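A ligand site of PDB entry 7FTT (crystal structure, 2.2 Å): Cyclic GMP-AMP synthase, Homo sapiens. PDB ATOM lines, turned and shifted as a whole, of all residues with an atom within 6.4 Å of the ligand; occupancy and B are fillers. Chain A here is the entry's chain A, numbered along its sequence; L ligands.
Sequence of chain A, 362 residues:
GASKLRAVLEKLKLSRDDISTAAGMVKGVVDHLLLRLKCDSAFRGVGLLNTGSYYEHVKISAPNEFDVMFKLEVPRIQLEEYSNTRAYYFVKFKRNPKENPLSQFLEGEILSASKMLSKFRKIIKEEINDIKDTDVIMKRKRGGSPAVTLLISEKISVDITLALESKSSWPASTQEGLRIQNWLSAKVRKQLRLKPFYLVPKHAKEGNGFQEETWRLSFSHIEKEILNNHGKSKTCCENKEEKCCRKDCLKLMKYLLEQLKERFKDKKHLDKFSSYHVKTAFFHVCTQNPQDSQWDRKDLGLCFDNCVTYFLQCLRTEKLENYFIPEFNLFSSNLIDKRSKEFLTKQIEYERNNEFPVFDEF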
ATOM      1  N   ARG A  86      16.426   6.216   6.011  1.00  0.00           N
ATOM      2  CA  ARG A  86      15.497   6.292   7.145  1.00  0.00           C
ATOM      3  C   ARG A  86      14.073   6.618   6.694  1.00  0.00           C
ATOM      4  O   ARG A  86      13.090   6.113   7.269  1.00  0.00           O
ATOM      5  CB  ARG A  86      15.972   7.321   8.179  1.00  0.00           C
ATOM      6  CG  ARG A  86      17.469   7.304   8.514  1.00  0.00           C
ATOM      7  CD  ARG A  86      17.787   6.727   9.895  1.00  0.00           C
ATOM      8  NE  ARG A  86      18.829   5.712   9.822  1.00  0.00           N
ATOM      9  CZ  ARG A  86      18.603   4.408   9.875  1.00  0.00           C
ATOM     10  NH1 ARG A  86      17.358   3.953  10.017  1.00  0.00           N
ATOM     11  NH2 ARG A  86      19.617   3.547   9.788  1.00  0.00           N
ATOM     12  N   ALA A  87      13.934   7.428   5.643  1.00  0.00           N
ATOM     13  CA  ALA A  87      12.633   7.929   5.209  1.00  0.00           C
ATOM     14  C   ALA A  87      12.026   7.209   4.009  1.00  0.00           C
ATOM     15  O   ALA A  87      10.813   7.228   3.853  1.00  0.00           O
ATOM     16  CB  ALA A  87      12.723   9.418   4.877  1.00  0.00           C
ATOM     17  N   TYR A  88      12.835   6.603   3.134  1.00  0.00           N
ATOM     18  CA  TYR A  88      12.298   6.027   1.899  1.00  0.00           C
ATOM     19  C   TYR A  88      12.459   4.500   1.906  1.00  0.00           C
ATOM     20  O   TYR A  88      13.456   3.976   2.425  1.00  0.00           O
ATOM     21  CB  TYR A  88      12.978   6.670   0.674  1.00  0.00           C
ATOM     22  CG  TYR A  88      12.753   8.184   0.562  1.00  0.00           C
ATOM     23  CD1 TYR A  88      11.685   8.706  -0.179  1.00  0.00           C
ATOM     24  CD2 TYR A  88      13.621   9.079   1.166  1.00  0.00           C
ATOM     25  CE1 TYR A  88      11.479  10.092  -0.288  1.00  0.00           C
ATOM     26  CE2 TYR A  88      13.427  10.469   1.064  1.00  0.00           C
ATOM     27  CZ  TYR A  88      12.356  10.965   0.342  1.00  0.00           C
ATOM     28  OH  TYR A  88      12.174  12.333   0.243  1.00  0.00           O
ATOM     29  N   ARG A 216       7.493   6.763   0.588  1.00  0.00           N
ATOM     30  CA  ARG A 216       7.780   7.444   1.833  1.00  0.00           C
ATOM     31  C   ARG A 216       6.490   7.631   2.610  1.00  0.00           C
ATOM     32  O   ARG A 216       5.404   7.636   2.024  1.00  0.00           O
ATOM     33  CB  ARG A 216       8.441   8.794   1.561  1.00  0.00           C
ATOM     34  CG  ARG A 216       7.621   9.686   0.670  1.00  0.00           C
ATOM     35  CD  ARG A 216       7.251  10.940   1.414  1.00  0.00           C
ATOM     36  NE  ARG A 216       6.404  11.844   0.643  1.00  0.00           N
ATOM     37  CZ  ARG A 216       5.256  12.327   1.075  1.00  0.00           C
ATOM     38  NH1 ARG A 216       4.557  13.145   0.305  1.00  0.00           N
ATOM     39  NH2 ARG A 216       4.785  11.967   2.268  1.00  0.00           N
ATOM     40  N   LEU A 217       6.614   7.799   3.923  1.00  0.00           N
ATOM     41  CA  LEU A 217       5.445   7.906   4.793  1.00  0.00           C
ATOM     42  C   LEU A 217       4.723   9.239   4.624  1.00  0.00           C
ATOM     43  O   LEU A 217       5.351  10.294   4.466  1.00  0.00           O
ATOM     44  CB  LEU A 217       5.858   7.768   6.257  1.00  0.00           C
ATOM     45  CG  LEU A 217       6.518   6.463   6.665  1.00  0.00           C
ATOM     46  CD1 LEU A 217       6.939   6.510   8.122  1.00  0.00           C
ATOM     47  CD2 LEU A 217       5.511   5.381   6.449  1.00  0.00           C
ATOM     48  N   SER A 218       3.397   9.203   4.724  1.00  0.00           N
ATOM     49  CA  SER A 218       2.566  10.408   4.781  1.00  0.00           C
ATOM     50  C   SER A 218       1.858  10.475   6.124  1.00  0.00           C
ATOM     51  O   SER A 218       1.293   9.464   6.577  1.00  0.00           O
ATOM     52  CB  SER A 218       1.540  10.425   3.660  1.00  0.00           C
ATOM     53  OG  SER A 218       0.635  11.518   3.854  1.00  0.00           O
ATOM     54  N   PHE A 219       1.902  11.650   6.773  1.00  0.00           N
ATOM     55  CA  PHE A 219       1.275  11.791   8.081  1.00  0.00           C
ATOM     56  C   PHE A 219       0.293  12.953   8.118  1.00  0.00           C
ATOM     57  O   PHE A 219       0.019  13.486   9.192  1.00  0.00           O
ATOM     58  CB  PHE A 219       2.305  11.952   9.190  1.00  0.00           C
ATOM     59  CG  PHE A 219       3.076  10.700   9.487  1.00  0.00           C
ATOM     60  CD1 PHE A 219       2.512   9.695  10.226  1.00  0.00           C
ATOM     61  CD2 PHE A 219       4.377  10.548   9.042  1.00  0.00           C
ATOM     62  CE1 PHE A 219       3.212   8.527  10.501  1.00  0.00           C
ATOM     63  CE2 PHE A 219       5.092   9.391   9.329  1.00  0.00           C
ATOM     64  CZ  PHE A 219       4.504   8.379  10.055  1.00  0.00           C
ATOM     65  N   SER A 220      -0.273  13.320   6.972  1.00  0.00           N
ATOM     66  CA  SER A 220      -1.327  14.320   6.983  1.00  0.00           C
ATOM     67  C   SER A 220      -2.445  13.956   7.963  1.00  0.00           C
ATOM     68  O   SER A 220      -3.000  14.839   8.634  1.00  0.00           O
ATOM     69  CB  SER A 220      -1.882  14.521   5.580  1.00  0.00           C
ATOM     70  OG  SER A 220      -0.952  15.260   4.811  1.00  0.00           O
ATOM     71  N   HIS A 221      -2.757  12.668   8.093  1.00  0.00           N
ATOM     72  CA  HIS A 221      -3.851  12.317   8.991  1.00  0.00           C
ATOM     73  C   HIS A 221      -3.477  12.575  10.438  1.00  0.00           C
ATOM     74  O   HIS A 221      -4.360  12.886  11.254  1.00  0.00           O
ATOM     75  CB  HIS A 221      -4.280  10.860   8.779  1.00  0.00           C
ATOM     76  CG  HIS A 221      -3.203   9.868   9.076  1.00  0.00           C
ATOM     77  ND1 HIS A 221      -2.076   9.732   8.283  1.00  0.00           N
ATOM     78  CD2 HIS A 221      -3.088   8.946  10.062  1.00  0.00           C
ATOM     79  CE1 HIS A 221      -1.306   8.779   8.776  1.00  0.00           C
ATOM     80  NE2 HIS A 221      -1.895   8.287   9.857  1.00  0.00           N
ATOM     81  N   GLU A 223      -1.115  14.987  11.504  1.00  0.00           N
ATOM     82  CA  GLU A 223      -1.149  16.446  11.575  1.00  0.00           C
ATOM     83  C   GLU A 223      -2.567  16.956  11.816  1.00  0.00           C
ATOM     84  O   GLU A 223      -2.822  17.703  12.771  1.00  0.00           O
ATOM     85  CB  GLU A 223      -0.586  17.010  10.271  1.00  0.00           C
ATOM     86  CG  GLU A 223      -1.176  18.321   9.854  1.00  0.00           C
ATOM     87  CD  GLU A 223      -0.571  18.862   8.576  1.00  0.00           C
ATOM     88  OE1 GLU A 223      -0.416  18.107   7.581  1.00  0.00           O
ATOM     89  OE2 GLU A 223      -0.236  20.051   8.567  1.00  0.00           O
ATOM     90  N   SER A 274       8.155  23.459   0.632  1.00  0.00           N
ATOM     91  CA  SER A 274       6.748  23.139   0.540  1.00  0.00           C
ATOM     92  C   SER A 274       6.076  23.495   1.865  1.00  0.00           C
ATOM     93  O   SER A 274       6.749  23.795   2.856  1.00  0.00           O
ATOM     94  CB  SER A 274       6.530  21.657   0.180  1.00  0.00           C
ATOM     95  OG  SER A 274       7.161  20.789   1.104  1.00  0.00           O
ATOM     96  N   SER A 275       4.746  23.484   1.880  1.00  0.00           N
ATOM     97  CA  SER A 275       4.070  23.752   3.150  1.00  0.00           C
ATOM     98  C   SER A 275       4.611  22.867   4.264  1.00  0.00           C
ATOM     99  O   SER A 275       4.589  23.268   5.433  1.00  0.00           O
ATOM    100  CB  SER A 275       2.563  23.540   3.003  1.00  0.00           C
ATOM    101  OG  SER A 275       2.286  22.206   2.565  1.00  0.00           O
ATOM    102  N   TYR A 276       5.152  21.720   3.917  1.00  0.00           N
ATOM    103  CA  TYR A 276       5.476  20.730   4.936  1.00  0.00           C
ATOM    104  C   TYR A 276       6.769  21.035   5.664  1.00  0.00           C
ATOM    105  O   TYR A 276       6.952  20.578   6.800  1.00  0.00           O
ATOM    106  CB  TYR A 276       5.478  19.361   4.259  1.00  0.00           C
ATOM    107  CG  TYR A 276       6.725  18.562   4.368  1.00  0.00           C
ATOM    108  CD1 TYR A 276       6.925  17.724   5.461  1.00  0.00           C
ATOM    109  CD2 TYR A 276       7.681  18.568   3.355  1.00  0.00           C
ATOM    110  CE1 TYR A 276       8.066  16.933   5.561  1.00  0.00           C
ATOM    111  CE2 TYR A 276       8.825  17.783   3.448  1.00  0.00           C
ATOM    112  CZ  TYR A 276       9.004  16.974   4.563  1.00  0.00           C
ATOM    113  OH  TYR A 276      10.118  16.180   4.701  1.00  0.00           O
ATOM    114  N   HIS A 277       7.681  21.816   5.074  1.00  0.00           N
ATOM    115  CA  HIS A 277       8.799  22.282   5.873  1.00  0.00           C
ATOM    116  C   HIS A 277       8.342  23.258   6.943  1.00  0.00           C
ATOM    117  O   HIS A 277       9.022  23.431   7.958  1.00  0.00           O
ATOM    118  CB  HIS A 277       9.843  22.963   4.999  1.00  0.00           C
ATOM    119  CG  HIS A 277      10.421  22.084   3.946  1.00  0.00           C
ATOM    120  ND1 HIS A 277       9.967  22.090   2.644  1.00  0.00           N
ATOM    121  CD2 HIS A 277      11.441  21.191   4.001  1.00  0.00           C
ATOM    122  CE1 HIS A 277      10.688  21.224   1.933  1.00  0.00           C
ATOM    123  NE2 HIS A 277      11.582  20.670   2.739  1.00  0.00           N
ATOM    124  N   LYS A 279       5.109  23.251   8.421  1.00  0.00           N
ATOM    125  CA  LYS A 279       4.458  22.444   9.446  1.00  0.00           C
ATOM    126  C   LYS A 279       5.489  21.770  10.339  1.00  0.00           C
ATOM    127  O   LYS A 279       5.360  21.781  11.575  1.00  0.00           O
ATOM    128  CB  LYS A 279       3.555  21.392   8.807  1.00  0.00           C
ATOM    129  CG  LYS A 279       2.191  21.871   8.349  1.00  0.00           C
ATOM    130  CD  LYS A 279       2.139  22.071   6.858  1.00  0.00           C
ATOM    131  CE  LYS A 279       1.138  21.154   6.143  1.00  0.00           C
ATOM    132  NZ  LYS A 279       1.582  19.725   6.080  1.00  0.00           N
ATOM    133  N   THR A 280       6.525  21.157   9.737  1.00  0.00           N
ATOM    134  CA  THR A 280       7.507  20.408  10.529  1.00  0.00           C
ATOM    135  C   THR A 280       8.163  21.302  11.559  1.00  0.00           C
ATOM    136  O   THR A 280       8.216  20.979  12.742  1.00  0.00           O
ATOM    137  CB  THR A 280       8.561  19.777   9.628  1.00  0.00           C
ATOM    138  OG1 THR A 280       8.005  18.602   9.039  1.00  0.00           O
ATOM    139  CG2 THR A 280       9.794  19.364  10.434  1.00  0.00           C
ATOM    140  N   PHE A 283       5.603  22.303  14.497  1.00  0.00           N
ATOM    141  CA  PHE A 283       5.366  21.323  15.554  1.00  0.00           C
ATOM    142  C   PHE A 283       6.557  21.202  16.500  1.00  0.00           C
ATOM    143  O   PHE A 283       6.375  20.846  17.676  1.00  0.00           O
ATOM    144  CB  PHE A 283       5.025  19.963  14.942  1.00  0.00           C
ATOM    145  CG  PHE A 283       3.635  19.910  14.382  1.00  0.00           C
ATOM    146  CD1 PHE A 283       2.558  20.363  15.129  1.00  0.00           C
ATOM    147  CD2 PHE A 283       3.395  19.424  13.115  1.00  0.00           C
ATOM    148  CE1 PHE A 283       1.271  20.329  14.631  1.00  0.00           C
ATOM    149  CE2 PHE A 283       2.102  19.377  12.619  1.00  0.00           C
ATOM    150  CZ  PHE A 283       1.037  19.835  13.372  1.00  0.00           C
ATOM    151  N   ASN A 322      12.944  15.865  10.597  1.00  0.00           N
ATOM    152  CA  ASN A 322      11.585  15.406  10.352  1.00  0.00           C
ATOM    153  C   ASN A 322      10.901  15.136  11.694  1.00  0.00           C
ATOM    154  O   ASN A 322      11.541  14.656  12.638  1.00  0.00           O
ATOM    155  CB  ASN A 322      11.562  14.142   9.497  1.00  0.00           C
ATOM    156  CG  ASN A 322      10.143  13.646   9.244  1.00  0.00           C
ATOM    157  OD1 ASN A 322       9.536  12.977  10.100  1.00  0.00           O
ATOM    158  ND2 ASN A 322       9.586  13.981   8.083  1.00  0.00           N
ATOM    159  N   TYR A 323       9.621  15.490  11.792  1.00  0.00           N
ATOM    160  CA  TYR A 323       8.965  15.395  13.079  1.00  0.00           C
ATOM    161  C   TYR A 323       8.676  13.966  13.486  1.00  0.00           C
ATOM    162  O   TYR A 323       8.448  13.704  14.667  1.00  0.00           O
ATOM    163  CB  TYR A 323       7.662  16.186  13.080  1.00  0.00           C
ATOM    164  CG  TYR A 323       7.158  16.539  14.476  1.00  0.00           C
ATOM    165  CD1 TYR A 323       7.913  17.376  15.322  1.00  0.00           C
ATOM    166  CD2 TYR A 323       5.930  16.082  14.942  1.00  0.00           C
ATOM    167  CE1 TYR A 323       7.445  17.738  16.602  1.00  0.00           C
ATOM    168  CE2 TYR A 323       5.453  16.427  16.232  1.00  0.00           C
ATOM    169  CZ  TYR A 323       6.226  17.250  17.052  1.00  0.00           C
ATOM    170  OH  TYR A 323       5.791  17.582  18.301  1.00  0.00           O
ATOM    171  N   PHE A 324       8.657  13.054  12.529  1.00  0.00           N
ATOM    172  CA  PHE A 324       8.294  11.679  12.783  1.00  0.00           C
ATOM    173  C   PHE A 324       9.446  10.726  12.640  1.00  0.00           C
ATOM    174  O   PHE A 324       9.409   9.644  13.240  1.00  0.00           O
ATOM    175  CB  PHE A 324       7.181  11.246  11.833  1.00  0.00           C
ATOM    176  CG  PHE A 324       5.870  11.943  12.068  1.00  0.00           C
ATOM    177  CD1 PHE A 324       5.016  11.502  13.047  1.00  0.00           C
ATOM    178  CD2 PHE A 324       5.487  13.012  11.271  1.00  0.00           C
ATOM    179  CE1 PHE A 324       3.765  12.134  13.265  1.00  0.00           C
ATOM    180  CE2 PHE A 324       4.243  13.654  11.472  1.00  0.00           C
ATOM    181  CZ  PHE A 324       3.382  13.206  12.482  1.00  0.00           C
ATOM    182  N   ILE A 325      10.468  11.088  11.869  1.00  0.00           N
ATOM    183  CA  ILE A 325      11.659  10.280  11.671  1.00  0.00           C
ATOM    184  C   ILE A 325      12.884  11.135  11.986  1.00  0.00           C
ATOM    185  O   ILE A 325      13.510  11.687  11.066  1.00  0.00           O
ATOM    186  CB  ILE A 325      11.747   9.736  10.240  1.00  0.00           C
ATOM    187  CG1 ILE A 325      10.391   9.171   9.785  1.00  0.00           C
ATOM    188  CG2 ILE A 325      12.816   8.682  10.153  1.00  0.00           C
ATOM    189  CD1 ILE A 325      10.186   9.152   8.264  1.00  0.00           C
ATOM    190  N   PHE A 328      16.357  12.153  10.123  1.00  0.00           N
ATOM    191  CA  PHE A 328      16.149  12.534   8.735  1.00  0.00           C
ATOM    192  C   PHE A 328      16.006  14.046   8.688  1.00  0.00           C
ATOM    193  O   PHE A 328      15.081  14.611   9.277  1.00  0.00           O
ATOM    194  CB  PHE A 328      14.922  11.823   8.163  1.00  0.00           C
ATOM    195  CG  PHE A 328      14.520  12.291   6.795  1.00  0.00           C
ATOM    196  CD1 PHE A 328      15.347  12.147   5.718  1.00  0.00           C
ATOM    197  CD2 PHE A 328      13.253  12.810   6.581  1.00  0.00           C
ATOM    198  CE1 PHE A 328      14.940  12.551   4.456  1.00  0.00           C
ATOM    199  CE2 PHE A 328      12.858  13.218   5.326  1.00  0.00           C
ATOM    200  CZ  PHE A 328      13.709  13.080   4.261  1.00  0.00           C
ATOM    201  N   LEU A 330      15.473  17.371   6.826  1.00  0.00           N
ATOM    202  CA  LEU A 330      14.918  17.966   5.615  1.00  0.00           C
ATOM    203  C   LEU A 330      15.772  19.106   5.051  1.00  0.00           C
ATOM    204  O   LEU A 330      15.489  19.565   3.929  1.00  0.00           O
ATOM    205  CB  LEU A 330      13.523  18.549   5.836  1.00  0.00           C
ATOM    206  CG  LEU A 330      12.624  18.109   6.959  1.00  0.00           C
ATOM    207  CD1 LEU A 330      11.386  18.957   6.884  1.00  0.00           C
ATOM    208  CD2 LEU A 330      12.289  16.664   6.751  1.00  0.00           C
HETATM  209  C1  LIG L   1       9.510  13.142   2.830  1.00  0.00           C
HETATM  210  C2  LIG L   1       8.281  13.750   3.052  1.00  0.00           C
HETATM  211  C3  LIG L   1       7.756  14.774   2.127  1.00  0.00           C
HETATM  212  C4  LIG L   1       8.335  15.303   0.967  1.00  0.00           C
HETATM  213  C5  LIG L   1       5.385  17.181   0.879  1.00  0.00           C
HETATM  214  C6  LIG L   1       4.852  15.726   8.322  1.00  0.00           C
HETATM  215  C7  LIG L   1       3.758  16.534   8.557  1.00  0.00           C
HETATM  216  C8  LIG L   1       2.576  16.362   7.889  1.00  0.00           C
HETATM  217  C9  LIG L   1       2.470  15.359   6.942  1.00  0.00           C
HETATM  218  C10 LIG L   1       7.523  13.374   4.155  1.00  0.00           C
HETATM  219  C11 LIG L   1       6.556  15.424   2.226  1.00  0.00           C
HETATM  220  C12 LIG L   1       3.558  14.530   6.669  1.00  0.00           C
HETATM  221  C13 LIG L   1       4.770  14.724   7.360  1.00  0.00           C
HETATM  222  C14 LIG L   1       6.033  13.940   7.215  1.00  0.00           C
HETATM  223  C15 LIG L   1       7.155  12.025   6.239  1.00  0.00           C
HETATM  224  C16 LIG L   1       7.985  12.422   5.052  1.00  0.00           C
HETATM  225  C17 LIG L   1       9.208  11.843   4.796  1.00  0.00           C
HETATM  226  C18 LIG L   1       9.981  12.183   3.714  1.00  0.00           C
HETATM  227  F1  LIG L   1       9.663  10.894   5.656  1.00  0.00           F
HETATM  228  N1  LIG L   1       6.468  16.252   1.193  1.00  0.00           N
HETATM  229  N2  LIG L   1       7.558  16.203   0.391  1.00  0.00           N
HETATM  230  N3  LIG L   1       6.021  12.937   6.339  1.00  0.00           N
HETATM  231  O1  LIG L   1       3.424  13.563   5.722  1.00  0.00           O
HETATM  232  O2  LIG L   1       7.027  14.209   7.886  1.00  0.00           O
HETATM  233 BR1  LIG L   1       3.895  17.869   9.902  1.00  0.00          BR
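An oxygen (O2) of the ligand is in hydrogen-bond range of the side-chain amide nitrogen (ND2) of Asn 322.
An oxygen (O1) of the ligand lies within hydrogen-bond range of the backbone NH (N) of Phe 219 (2.7 Å).
The backbone carbonyl oxygen (O) of Leu 217 lies close to a nitrogen (N3) of the ligand (3.3 Å).
Ala 87 touches the ligand.
OH of Tyr 88 touches C1 of the ligand (3.8 Å).
Arg 216 touches the ligand (CD to C2, 3.4 Å).
Ser 218 touches the ligand.
Ser 220 touches the ligand (N to C9, 3.4 Å).
Glu 223 touches the ligand (OE1 to C8, 3.5 Å).
Tyr 276 touches the ligand (CD2 to N1, 3.4 Å).
CB of Lys 279 touches BR1 of the ligand, at 3.7 Å.
Phe 283 touches the ligand (CE2 to BR1, 3.6 Å).
Phe 324 touches the ligand.
CD1 of Ile 325 touches F1 of the ligand, 3.2 Å away.
Phe 328 touches the ligand (CE2 to C18, 3.5 Å).
Hydrophobic or aromatic side chains that line the ligand: Ala 87, Phe 219, Tyr 276, Phe 283, Phe 324, Ile 325 and Phe 328.
15 residues have an atom within 4 Å of the ligand: Ala 87, Tyr 88, Arg 216, Leu 217, Ser 218, Phe 219, Ser 220, Glu 223, Tyr 276, Lys 279, Phe 283, Asn 322, Phe 324, Ile 325 and Phe 328.
The nearest printed residue that does not touch the ligand is Ser 274 (4.03 Å).
The side-chain amide oxygen (OD1) of Asn 322 is in hydrogen-bond range of the backbone NH (N) of Ile 325 (2.8 Å).
The backbone carbonyl oxygen (O) of Phe 328 sits at hydrogen-bond distance from the backbone NH (N) of Asn 322 (2.8 Å).
The side-chain amide oxygen (OD1) of Asn 322 sits at hydrogen-bond distance from the backbone NH (N) of Phe 324, at 2.6 Å.
The backbone carbonyl oxygen of Tyr 276 sits at hydrogen-bond distance from the side-chain hydroxyl of Thr 280, 3.2 Å away.
OE1 of Glu 223 is in salt-bridge range of NZ of Lys 279 (3.0 Å).
OH of Tyr 323 sits at hydrogen-bond distance from O of Phe 283 (3.4 Å).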
